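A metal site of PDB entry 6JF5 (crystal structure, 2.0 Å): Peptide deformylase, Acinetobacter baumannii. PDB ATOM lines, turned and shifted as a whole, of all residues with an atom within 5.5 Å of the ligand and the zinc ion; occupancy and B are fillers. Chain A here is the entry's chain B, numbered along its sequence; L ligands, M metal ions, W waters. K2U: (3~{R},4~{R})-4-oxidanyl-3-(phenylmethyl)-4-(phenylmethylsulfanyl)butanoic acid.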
ATOM      1  N   ASN A  46     -22.141  37.200 -23.418  1.00  0.00           N
ATOM      2  CA  ASN A  46     -20.947  36.524 -22.864  1.00  0.00           C
ATOM      3  C   ASN A  46     -20.563  35.308 -23.715  1.00  0.00           C
ATOM      4  O   ASN A  46     -20.047  34.308 -23.133  1.00  0.00           O
ATOM      5  CB  ASN A  46     -21.153  36.069 -21.418  1.00  0.00           C
ATOM      6  CG  ASN A  46     -21.192  37.219 -20.453  1.00  0.00           C
ATOM      7  OD1 ASN A  46     -20.421  38.166 -20.580  1.00  0.00           O
ATOM      8  ND2 ASN A  46     -22.073  37.135 -19.465  1.00  0.00           N
ATOM      9  N   GLY A  47     -20.727  35.401 -25.036  1.00  0.00           N
ATOM     10  CA  GLY A  47     -20.397  34.282 -25.932  1.00  0.00           C
ATOM     11  C   GLY A  47     -18.931  34.244 -26.313  1.00  0.00           C
ATOM     12  O   GLY A  47     -18.240  35.265 -26.176  1.00  0.00           O
ATOM     13  N   VAL A  48     -18.462  33.143 -26.885  1.00  0.00           N
ATOM     14  CA  VAL A  48     -17.081  33.035 -27.433  1.00  0.00           C
ATOM     15  C   VAL A  48     -17.109  32.839 -28.959  1.00  0.00           C
ATOM     16  O   VAL A  48     -16.049  32.655 -29.583  1.00  0.00           O
ATOM     17  CB  VAL A  48     -16.346  31.894 -26.714  1.00  0.00           C
ATOM     18  CG1 VAL A  48     -16.039  32.326 -25.275  1.00  0.00           C
ATOM     19  CG2 VAL A  48     -17.170  30.613 -26.755  1.00  0.00           C
ATOM     20  N   GLY A  49     -18.306  32.867 -29.522  1.00  0.00           N
ATOM     21  CA  GLY A  49     -18.498  32.772 -30.979  1.00  0.00           C
ATOM     22  C   GLY A  49     -19.922  33.122 -31.340  1.00  0.00           C
ATOM     23  O   GLY A  49     -20.784  33.186 -30.428  1.00  0.00           O
ATOM     24  N   ILE A  50     -20.185  33.334 -32.622  1.00  0.00           N
ATOM     25  CA  ILE A  50     -21.543  33.591 -33.122  1.00  0.00           C
ATOM     26  C   ILE A  50     -21.541  33.327 -34.618  1.00  0.00           C
ATOM     27  O   ILE A  50     -20.464  33.402 -35.211  1.00  0.00           O
ATOM     28  CB  ILE A  50     -22.052  34.987 -32.701  1.00  0.00           C
ATOM     29  CG1 ILE A  50     -23.544  35.116 -32.964  1.00  0.00           C
ATOM     30  CG2 ILE A  50     -21.223  36.108 -33.310  1.00  0.00           C
ATOM     31  CD1 ILE A  50     -24.202  36.291 -32.304  1.00  0.00           C
ATOM     32  N   ALA A  51     -22.683  32.937 -35.186  1.00  0.00           N
ATOM     33  CA  ALA A  51     -22.861  32.694 -36.615  1.00  0.00           C
ATOM     34  C   ALA A  51     -24.034  33.566 -37.070  1.00  0.00           C
ATOM     35  O   ALA A  51     -24.976  33.715 -36.321  1.00  0.00           O
ATOM     36  CB  ALA A  51     -23.133  31.212 -36.843  1.00  0.00           C
ATOM     37  N   GLN A  54     -27.966  32.898 -36.409  1.00  0.00           N
ATOM     38  CA  GLN A  54     -28.392  33.126 -35.008  1.00  0.00           C
ATOM     39  C   GLN A  54     -28.984  34.511 -34.820  1.00  0.00           C
ATOM     40  O   GLN A  54     -29.755  34.667 -33.878  1.00  0.00           O
ATOM     41  CB  GLN A  54     -27.213  32.943 -34.062  1.00  0.00           C
ATOM     42  CG  GLN A  54     -26.752  31.516 -33.937  1.00  0.00           C
ATOM     43  CD  GLN A  54     -25.665  31.380 -32.903  1.00  0.00           C
ATOM     44  OE1 GLN A  54     -24.487  31.720 -33.153  1.00  0.00           O
ATOM     45  NE2 GLN A  54     -26.089  30.922 -31.722  1.00  0.00           N
ATOM     46  N   ARG A  67     -11.839  32.183 -24.563  1.00  0.00           N
ATOM     47  CA  ARG A  67     -11.338  32.611 -23.229  1.00  0.00           C
ATOM     48  C   ARG A  67     -11.183  31.387 -22.335  1.00  0.00           C
ATOM     49  O   ARG A  67     -11.848  30.373 -22.558  1.00  0.00           O
ATOM     50  CB  ARG A  67     -12.231  33.725 -22.672  1.00  0.00           C
ATOM     51  CG  ARG A  67     -13.692  33.344 -22.496  1.00  0.00           C
ATOM     52  CD  ARG A  67     -14.344  34.124 -21.391  1.00  0.00           C
ATOM     53  NE  ARG A  67     -15.701  33.655 -21.178  1.00  0.00           N
ATOM     54  CZ  ARG A  67     -16.770  34.109 -21.826  1.00  0.00           C
ATOM     55  NH1 ARG A  67     -17.965  33.598 -21.576  1.00  0.00           N
ATOM     56  NH2 ARG A  67     -16.657  35.076 -22.715  1.00  0.00           N
ATOM     57  N   ASN A  69     -11.729  29.010 -19.121  1.00  0.00           N
ATOM     58  CA  ASN A  69     -12.934  28.719 -18.299  1.00  0.00           C
ATOM     59  C   ASN A  69     -12.640  27.465 -17.484  1.00  0.00           C
ATOM     60  O   ASN A  69     -11.553  26.879 -17.626  1.00  0.00           O
ATOM     61  CB  ASN A  69     -14.189  28.615 -19.175  1.00  0.00           C
ATOM     62  CG  ASN A  69     -14.072  27.584 -20.284  1.00  0.00           C
ATOM     63  OD1 ASN A  69     -13.568  27.886 -21.362  1.00  0.00           O
ATOM     64  ND2 ASN A  69     -14.518  26.366 -20.032  1.00  0.00           N
ATOM     65  N   TYR A  72     -11.683  24.389 -19.886  1.00  0.00           N
ATOM     66  CA  TYR A  72     -10.406  24.588 -20.631  1.00  0.00           C
ATOM     67  C   TYR A  72      -9.641  25.760 -20.026  1.00  0.00           C
ATOM     68  O   TYR A  72      -9.677  26.873 -20.547  1.00  0.00           O
ATOM     69  CB  TYR A  72     -10.657  24.864 -22.120  1.00  0.00           C
ATOM     70  CG  TYR A  72     -11.799  24.125 -22.758  1.00  0.00           C
ATOM     71  CD1 TYR A  72     -13.111  24.500 -22.520  1.00  0.00           C
ATOM     72  CD2 TYR A  72     -11.567  23.077 -23.640  1.00  0.00           C
ATOM     73  CE1 TYR A  72     -14.174  23.837 -23.124  1.00  0.00           C
ATOM     74  CE2 TYR A  72     -12.613  22.400 -24.247  1.00  0.00           C
ATOM     75  CZ  TYR A  72     -13.921  22.780 -23.978  1.00  0.00           C
ATOM     76  OH  TYR A  72     -14.974  22.140 -24.567  1.00  0.00           O
ATOM     77  N   GLU A  99     -17.124  20.461 -23.351  1.00  0.00           N
ATOM     78  CA  GLU A  99     -18.330  21.176 -22.908  1.00  0.00           C
ATOM     79  C   GLU A  99     -18.664  22.272 -23.936  1.00  0.00           C
ATOM     80  O   GLU A  99     -17.794  23.089 -24.281  1.00  0.00           O
ATOM     81  CB  GLU A  99     -18.112  21.689 -21.490  1.00  0.00           C
ATOM     82  CG  GLU A  99     -18.742  23.041 -21.198  1.00  0.00           C
ATOM     83  CD  GLU A  99     -19.956  23.010 -20.283  1.00  0.00           C
ATOM     84  OE1 GLU A  99     -20.867  22.185 -20.556  1.00  0.00           O
ATOM     85  OE2 GLU A  99     -19.986  23.802 -19.298  1.00  0.00           O
ATOM     86  N   GLU A 100     -19.902  22.294 -24.405  1.00  0.00           N
ATOM     87  CA  GLU A 100     -20.386  23.337 -25.346  1.00  0.00           C
ATOM     88  C   GLU A 100     -21.666  23.913 -24.772  1.00  0.00           C
ATOM     89  O   GLU A 100     -22.395  23.185 -24.076  1.00  0.00           O
ATOM     90  CB  GLU A 100     -20.625  22.769 -26.744  1.00  0.00           C
ATOM     91  CG  GLU A 100     -19.328  22.314 -27.406  1.00  0.00           C
ATOM     92  CD  GLU A 100     -19.340  22.148 -28.920  1.00  0.00           C
ATOM     93  OE1 GLU A 100     -20.310  22.623 -29.585  1.00  0.00           O
ATOM     94  OE2 GLU A 100     -18.372  21.567 -29.435  1.00  0.00           O
ATOM     95  N   GLY A 101     -21.886  25.191 -25.057  1.00  0.00           N
ATOM     96  CA  GLY A 101     -23.188  25.851 -24.950  1.00  0.00           C
ATOM     97  C   GLY A 101     -23.540  26.480 -26.275  1.00  0.00           C
ATOM     98  O   GLY A 101     -22.694  26.396 -27.214  1.00  0.00           O
ATOM     99  N   CYS A 102     -24.690  27.112 -26.343  1.00  0.00           N
ATOM    100  CA  CYS A 102     -25.170  27.828 -27.545  1.00  0.00           C
ATOM    101  C   CYS A 102     -26.061  29.002 -27.142  1.00  0.00           C
ATOM    102  O   CYS A 102     -26.964  28.797 -26.314  1.00  0.00           O
ATOM    103  CB  CYS A 102     -25.914  26.830 -28.410  1.00  0.00           C
ATOM    104  SG  CYS A 102     -26.304  27.440 -30.056  1.00  0.00           S
ATOM    105  N   LEU A 103     -25.862  30.163 -27.749  1.00  0.00           N
ATOM    106  CA  LEU A 103     -26.771  31.319 -27.557  1.00  0.00           C
ATOM    107  C   LEU A 103     -28.188  30.948 -28.016  1.00  0.00           C
ATOM    108  O   LEU A 103     -29.130  31.622 -27.566  1.00  0.00           O
ATOM    109  CB  LEU A 103     -26.323  32.538 -28.360  1.00  0.00           C
ATOM    110  CG  LEU A 103     -24.874  32.966 -28.167  1.00  0.00           C
ATOM    111  CD1 LEU A 103     -24.429  33.920 -29.267  1.00  0.00           C
ATOM    112  CD2 LEU A 103     -24.704  33.584 -26.797  1.00  0.00           C
ATOM    113  N   SER A 104     -28.335  30.012 -28.947  1.00  0.00           N
ATOM    114  CA  SER A 104     -29.649  29.631 -29.519  1.00  0.00           C
ATOM    115  C   SER A 104     -30.278  28.501 -28.687  1.00  0.00           C
ATOM    116  O   SER A 104     -31.441  28.162 -28.953  1.00  0.00           O
ATOM    117  CB  SER A 104     -29.555  29.251 -30.968  1.00  0.00           C
ATOM    118  OG  SER A 104     -29.150  30.366 -31.748  1.00  0.00           O
ATOM    119  N   ARG A 109     -26.341  22.796 -21.667  1.00  0.00           N
ATOM    120  CA  ARG A 109     -24.914  22.626 -22.023  1.00  0.00           C
ATOM    121  C   ARG A 109     -24.673  21.137 -22.193  1.00  0.00           C
ATOM    122  O   ARG A 109     -25.395  20.352 -21.583  1.00  0.00           O
ATOM    123  CB  ARG A 109     -23.979  23.204 -20.960  1.00  0.00           C
ATOM    124  CG  ARG A 109     -24.385  24.548 -20.377  1.00  0.00           C
ATOM    125  CD  ARG A 109     -23.891  25.738 -21.152  1.00  0.00           C
ATOM    126  NE  ARG A 109     -22.462  25.977 -20.986  1.00  0.00           N
ATOM    127  CZ  ARG A 109     -21.893  26.631 -19.967  1.00  0.00           C
ATOM    128  NH1 ARG A 109     -22.625  27.135 -18.992  1.00  0.00           N
ATOM    129  NH2 ARG A 109     -20.577  26.787 -19.956  1.00  0.00           N
ATOM    130  N   PHE A 137      -9.998  24.482 -27.708  1.00  0.00           N
ATOM    131  CA  PHE A 137     -11.306  25.127 -27.488  1.00  0.00           C
ATOM    132  C   PHE A 137     -11.721  25.907 -28.740  1.00  0.00           C
ATOM    133  O   PHE A 137     -12.835  25.763 -29.204  1.00  0.00           O
ATOM    134  CB  PHE A 137     -11.267  25.994 -26.221  1.00  0.00           C
ATOM    135  CG  PHE A 137     -12.584  26.633 -25.859  1.00  0.00           C
ATOM    136  CD1 PHE A 137     -13.765  25.904 -25.869  1.00  0.00           C
ATOM    137  CD2 PHE A 137     -12.618  27.942 -25.398  1.00  0.00           C
ATOM    138  CE1 PHE A 137     -14.955  26.488 -25.470  1.00  0.00           C
ATOM    139  CE2 PHE A 137     -13.808  28.526 -24.999  1.00  0.00           C
ATOM    140  CZ  PHE A 137     -14.972  27.798 -25.050  1.00  0.00           C
ATOM    141  N   ARG A 140     -13.055  23.717 -31.421  1.00  0.00           N
ATOM    142  CA  ARG A 140     -14.443  23.366 -31.021  1.00  0.00           C
ATOM    143  C   ARG A 140     -15.379  24.507 -31.431  1.00  0.00           C
ATOM    144  O   ARG A 140     -16.498  24.231 -31.953  1.00  0.00           O
ATOM    145  CB  ARG A 140     -14.507  23.034 -29.518  1.00  0.00           C
ATOM    146  N   ILE A 141     -14.986  25.747 -31.191  1.00  0.00           N
ATOM    147  CA  ILE A 141     -15.871  26.912 -31.463  1.00  0.00           C
ATOM    148  C   ILE A 141     -16.044  27.009 -32.981  1.00  0.00           C
ATOM    149  O   ILE A 141     -17.149  27.284 -33.434  1.00  0.00           O
ATOM    150  CB  ILE A 141     -15.304  28.206 -30.855  1.00  0.00           C
ATOM    151  CG1 ILE A 141     -15.150  28.086 -29.331  1.00  0.00           C
ATOM    152  CG2 ILE A 141     -16.173  29.390 -31.294  1.00  0.00           C
ATOM    153  CD1 ILE A 141     -14.204  29.070 -28.770  1.00  0.00           C
ATOM    154  N   HIS A 144     -18.473  24.340 -34.160  1.00  0.00           N
ATOM    155  CA  HIS A 144     -19.831  24.714 -33.680  1.00  0.00           C
ATOM    156  C   HIS A 144     -20.440  25.784 -34.614  1.00  0.00           C
ATOM    157  O   HIS A 144     -21.599  25.684 -35.048  1.00  0.00           O
ATOM    158  CB  HIS A 144     -19.712  25.150 -32.213  1.00  0.00           C
ATOM    159  CG  HIS A 144     -21.020  25.627 -31.647  1.00  0.00           C
ATOM    160  ND1 HIS A 144     -21.642  24.976 -30.601  1.00  0.00           N
ATOM    161  CD2 HIS A 144     -21.797  26.663 -31.964  1.00  0.00           C
ATOM    162  CE1 HIS A 144     -22.735  25.619 -30.277  1.00  0.00           C
ATOM    163  NE2 HIS A 144     -22.866  26.654 -31.115  1.00  0.00           N
ATOM    164  N   GLU A 145     -19.657  26.804 -34.963  1.00  0.00           N
ATOM    165  CA  GLU A 145     -20.119  27.939 -35.796  1.00  0.00           C
ATOM    166  C   GLU A 145     -20.366  27.496 -37.243  1.00  0.00           C
ATOM    167  O   GLU A 145     -21.373  27.935 -37.812  1.00  0.00           O
ATOM    168  CB  GLU A 145     -19.136  29.110 -35.734  1.00  0.00           C
ATOM    169  CG  GLU A 145     -18.897  29.628 -34.327  1.00  0.00           C
ATOM    170  CD  GLU A 145     -20.128  30.005 -33.519  1.00  0.00           C
ATOM    171  OE1 GLU A 145     -21.167  30.331 -34.113  1.00  0.00           O
ATOM    172  OE2 GLU A 145     -20.043  29.944 -32.264  1.00  0.00           O
ATOM    173  N   HIS A 148     -23.582  25.867 -37.489  1.00  0.00           N
ATOM    174  CA  HIS A 148     -24.691  26.848 -37.558  1.00  0.00           C
ATOM    175  C   HIS A 148     -24.964  27.257 -39.014  1.00  0.00           C
ATOM    176  O   HIS A 148     -26.149  27.390 -39.358  1.00  0.00           O
ATOM    177  CB  HIS A 148     -24.465  28.116 -36.724  1.00  0.00           C
ATOM    178  CG  HIS A 148     -24.880  28.010 -35.299  1.00  0.00           C
ATOM    179  ND1 HIS A 148     -26.139  27.576 -34.915  1.00  0.00           N
ATOM    180  CD2 HIS A 148     -24.203  28.268 -34.157  1.00  0.00           C
ATOM    181  CE1 HIS A 148     -26.219  27.588 -33.602  1.00  0.00           C
ATOM    182  NE2 HIS A 148     -25.058  28.031 -33.117  1.00  0.00           N
ATOM    183  N   PHE A 154     -25.736  21.940 -31.678  1.00  0.00           N
ATOM    184  CA  PHE A 154     -24.802  21.013 -30.984  1.00  0.00           C
ATOM    185  C   PHE A 154     -25.553  19.837 -30.345  1.00  0.00           C
ATOM    186  O   PHE A 154     -24.958  18.772 -30.234  1.00  0.00           O
ATOM    187  CB  PHE A 154     -23.939  21.776 -29.992  1.00  0.00           C
ATOM    188  CG  PHE A 154     -24.594  22.140 -28.683  1.00  0.00           C
ATOM    189  CD1 PHE A 154     -25.383  23.284 -28.557  1.00  0.00           C
ATOM    190  CD2 PHE A 154     -24.372  21.363 -27.555  1.00  0.00           C
ATOM    191  CE1 PHE A 154     -25.936  23.632 -27.337  1.00  0.00           C
ATOM    192  CE2 PHE A 154     -24.938  21.704 -26.345  1.00  0.00           C
ATOM    193  CZ  PHE A 154     -25.716  22.836 -26.235  1.00  0.00           C
HETATM  194  O22 K2U L   1     -22.418  29.802 -31.315  1.00  0.00           O
HETATM  195  C1  K2U L   1     -22.852  29.990 -30.223  1.00  0.00           C
HETATM  196  O21 K2U L   1     -24.025  29.542 -29.919  1.00  0.00           O
HETATM  197  C2  K2U L   1     -22.033  30.641 -29.193  1.00  0.00           C
HETATM  198  C3  K2U L   1     -21.467  29.639 -28.193  1.00  0.00           C
HETATM  199  C4  K2U L   1     -20.132  29.135 -28.777  1.00  0.00           C
HETATM  200  C5  K2U L   1     -19.440  27.887 -28.238  1.00  0.00           C
HETATM  201  C6  K2U L   1     -19.125  27.733 -26.885  1.00  0.00           C
HETATM  202  C7  K2U L   1     -18.480  26.595 -26.416  1.00  0.00           C
HETATM  203  C8  K2U L   1     -18.110  25.581 -27.294  1.00  0.00           C
HETATM  204  C9  K2U L   1     -18.428  25.711 -28.648  1.00  0.00           C
HETATM  205  C10 K2U L   1     -19.070  26.867 -29.091  1.00  0.00           C
HETATM  206  C11 K2U L   1     -21.504  30.543 -26.927  1.00  0.00           C
HETATM  207  O12 K2U L   1     -20.253  31.095 -26.635  1.00  0.00           O
HETATM  208  S13 K2U L   1     -22.193  29.707 -25.558  1.00  0.00           S
HETATM  209  C14 K2U L   1     -21.572  30.277 -23.982  1.00  0.00           C
HETATM  210  C15 K2U L   1     -20.275  29.597 -23.564  1.00  0.00           C
HETATM  211  C16 K2U L   1     -20.240  28.218 -23.382  1.00  0.00           C
HETATM  212  C17 K2U L   1     -19.049  27.588 -22.997  1.00  0.00           C
HETATM  213  C18 K2U L   1     -17.893  28.342 -22.784  1.00  0.00           C
HETATM  214  C19 K2U L   1     -17.920  29.717 -22.963  1.00  0.00           C
HETATM  215  C20 K2U L   1     -19.112  30.355 -23.363  1.00  0.00           C
HETATM  216 ZN    ZN M   1     -24.381  28.008 -31.088  1.00  0.00          ZN
HETATM  217  O   HOH W   1     -25.538  24.794 -31.677  1.00  0.00           O
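O of Gly 101 lies close to S13 of the ligand, 3.7 Å away.
Residues that only touch the ligand: Gly 49, Gly 47, Glu 100, Arg 109, Phe 137, Arg 67, Glu 99 and Ile 141.
Hydrophobic or aromatic side chains that line the ligand: Val 48, Leu 103, Phe 137, His 144 and His 148.
16 residues have an atom within 4 Å of the ligand: Gly 47, Val 48, Gly 49, Gln 54, Arg 67, Glu 99, Glu 100, Gly 101, Cys 102, Leu 103, Arg 109, Phe 137, Ile 141, His 144, Glu 145 and His 148.
The nearest printed residue that does not touch the ligand is Asn 46 (4.1 Å).
The side-chain carboxylate (OE1) of Glu 100 is in hydrogen-bond range of a ring nitrogen (ND1) of His 144 (2.9 Å).
NE2 of His 148 lies close to NE2 of Gln 54, at 3.4 Å.
The side-chain sulfur (SG) of Cys 102 sits close to the backbone NH (N) of Ser 104 (3.5 Å).
OE2 of Glu 145 lies within hydrogen-bond range of N of Ile 50 (3.4 Å).
The backbone NH (N) of Ala 51 sits at hydrogen-bond distance from the side-chain carboxylate (OE1) of Glu 145 (3.2 Å).
The side-chain hydroxyl (OG) of Ser 104 is in hydrogen-bond range of the side-chain amide nitrogen (NE2) of Gln 54 (3.1 Å).
OE1 of Gln 54 lies within hydrogen-bond range of N of Ala 51 (3.0 Å).
O of Arg 67 lies close to OD1 of Asn 69 (3.3 Å).
The zinc ion is bound by O21 of the ligand, NE2 of His 144, NE2 of His 148 and SG of Cys 102.
Slightly farther from the zinc ion lies an oxygen (O22) of the ligand (2.7 Å).
The backbone NH (N) of Cys 102 sits close to a sulfur (S13) of the ligand (3.7 Å).
OE2 of Glu 145 sits close to O22 of the ligand (2.6 Å).
N of Val 48 lies within hydrogen-bond range of O12 of the ligand (2.7 Å).
N of Leu 103 sits close to O21 of the ligand, at 2.9 Å.
The side-chain amide oxygen of Gln 54 sits close to an oxygen (O22) of the ligand (3.4 Å).
Merely in contact with the zinc ion: Gln 54 (3.4 Å).
Four residues have an atom within 4 Å of the zinc ion: Gln 54, Cys 102, His 144 and His 148.
Along chain A the residues within 4 Å of the zinc ion span positions 54 to 148.
The nearest printed residue that does not touch the zinc ion is Leu 103 (4.2 Å).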
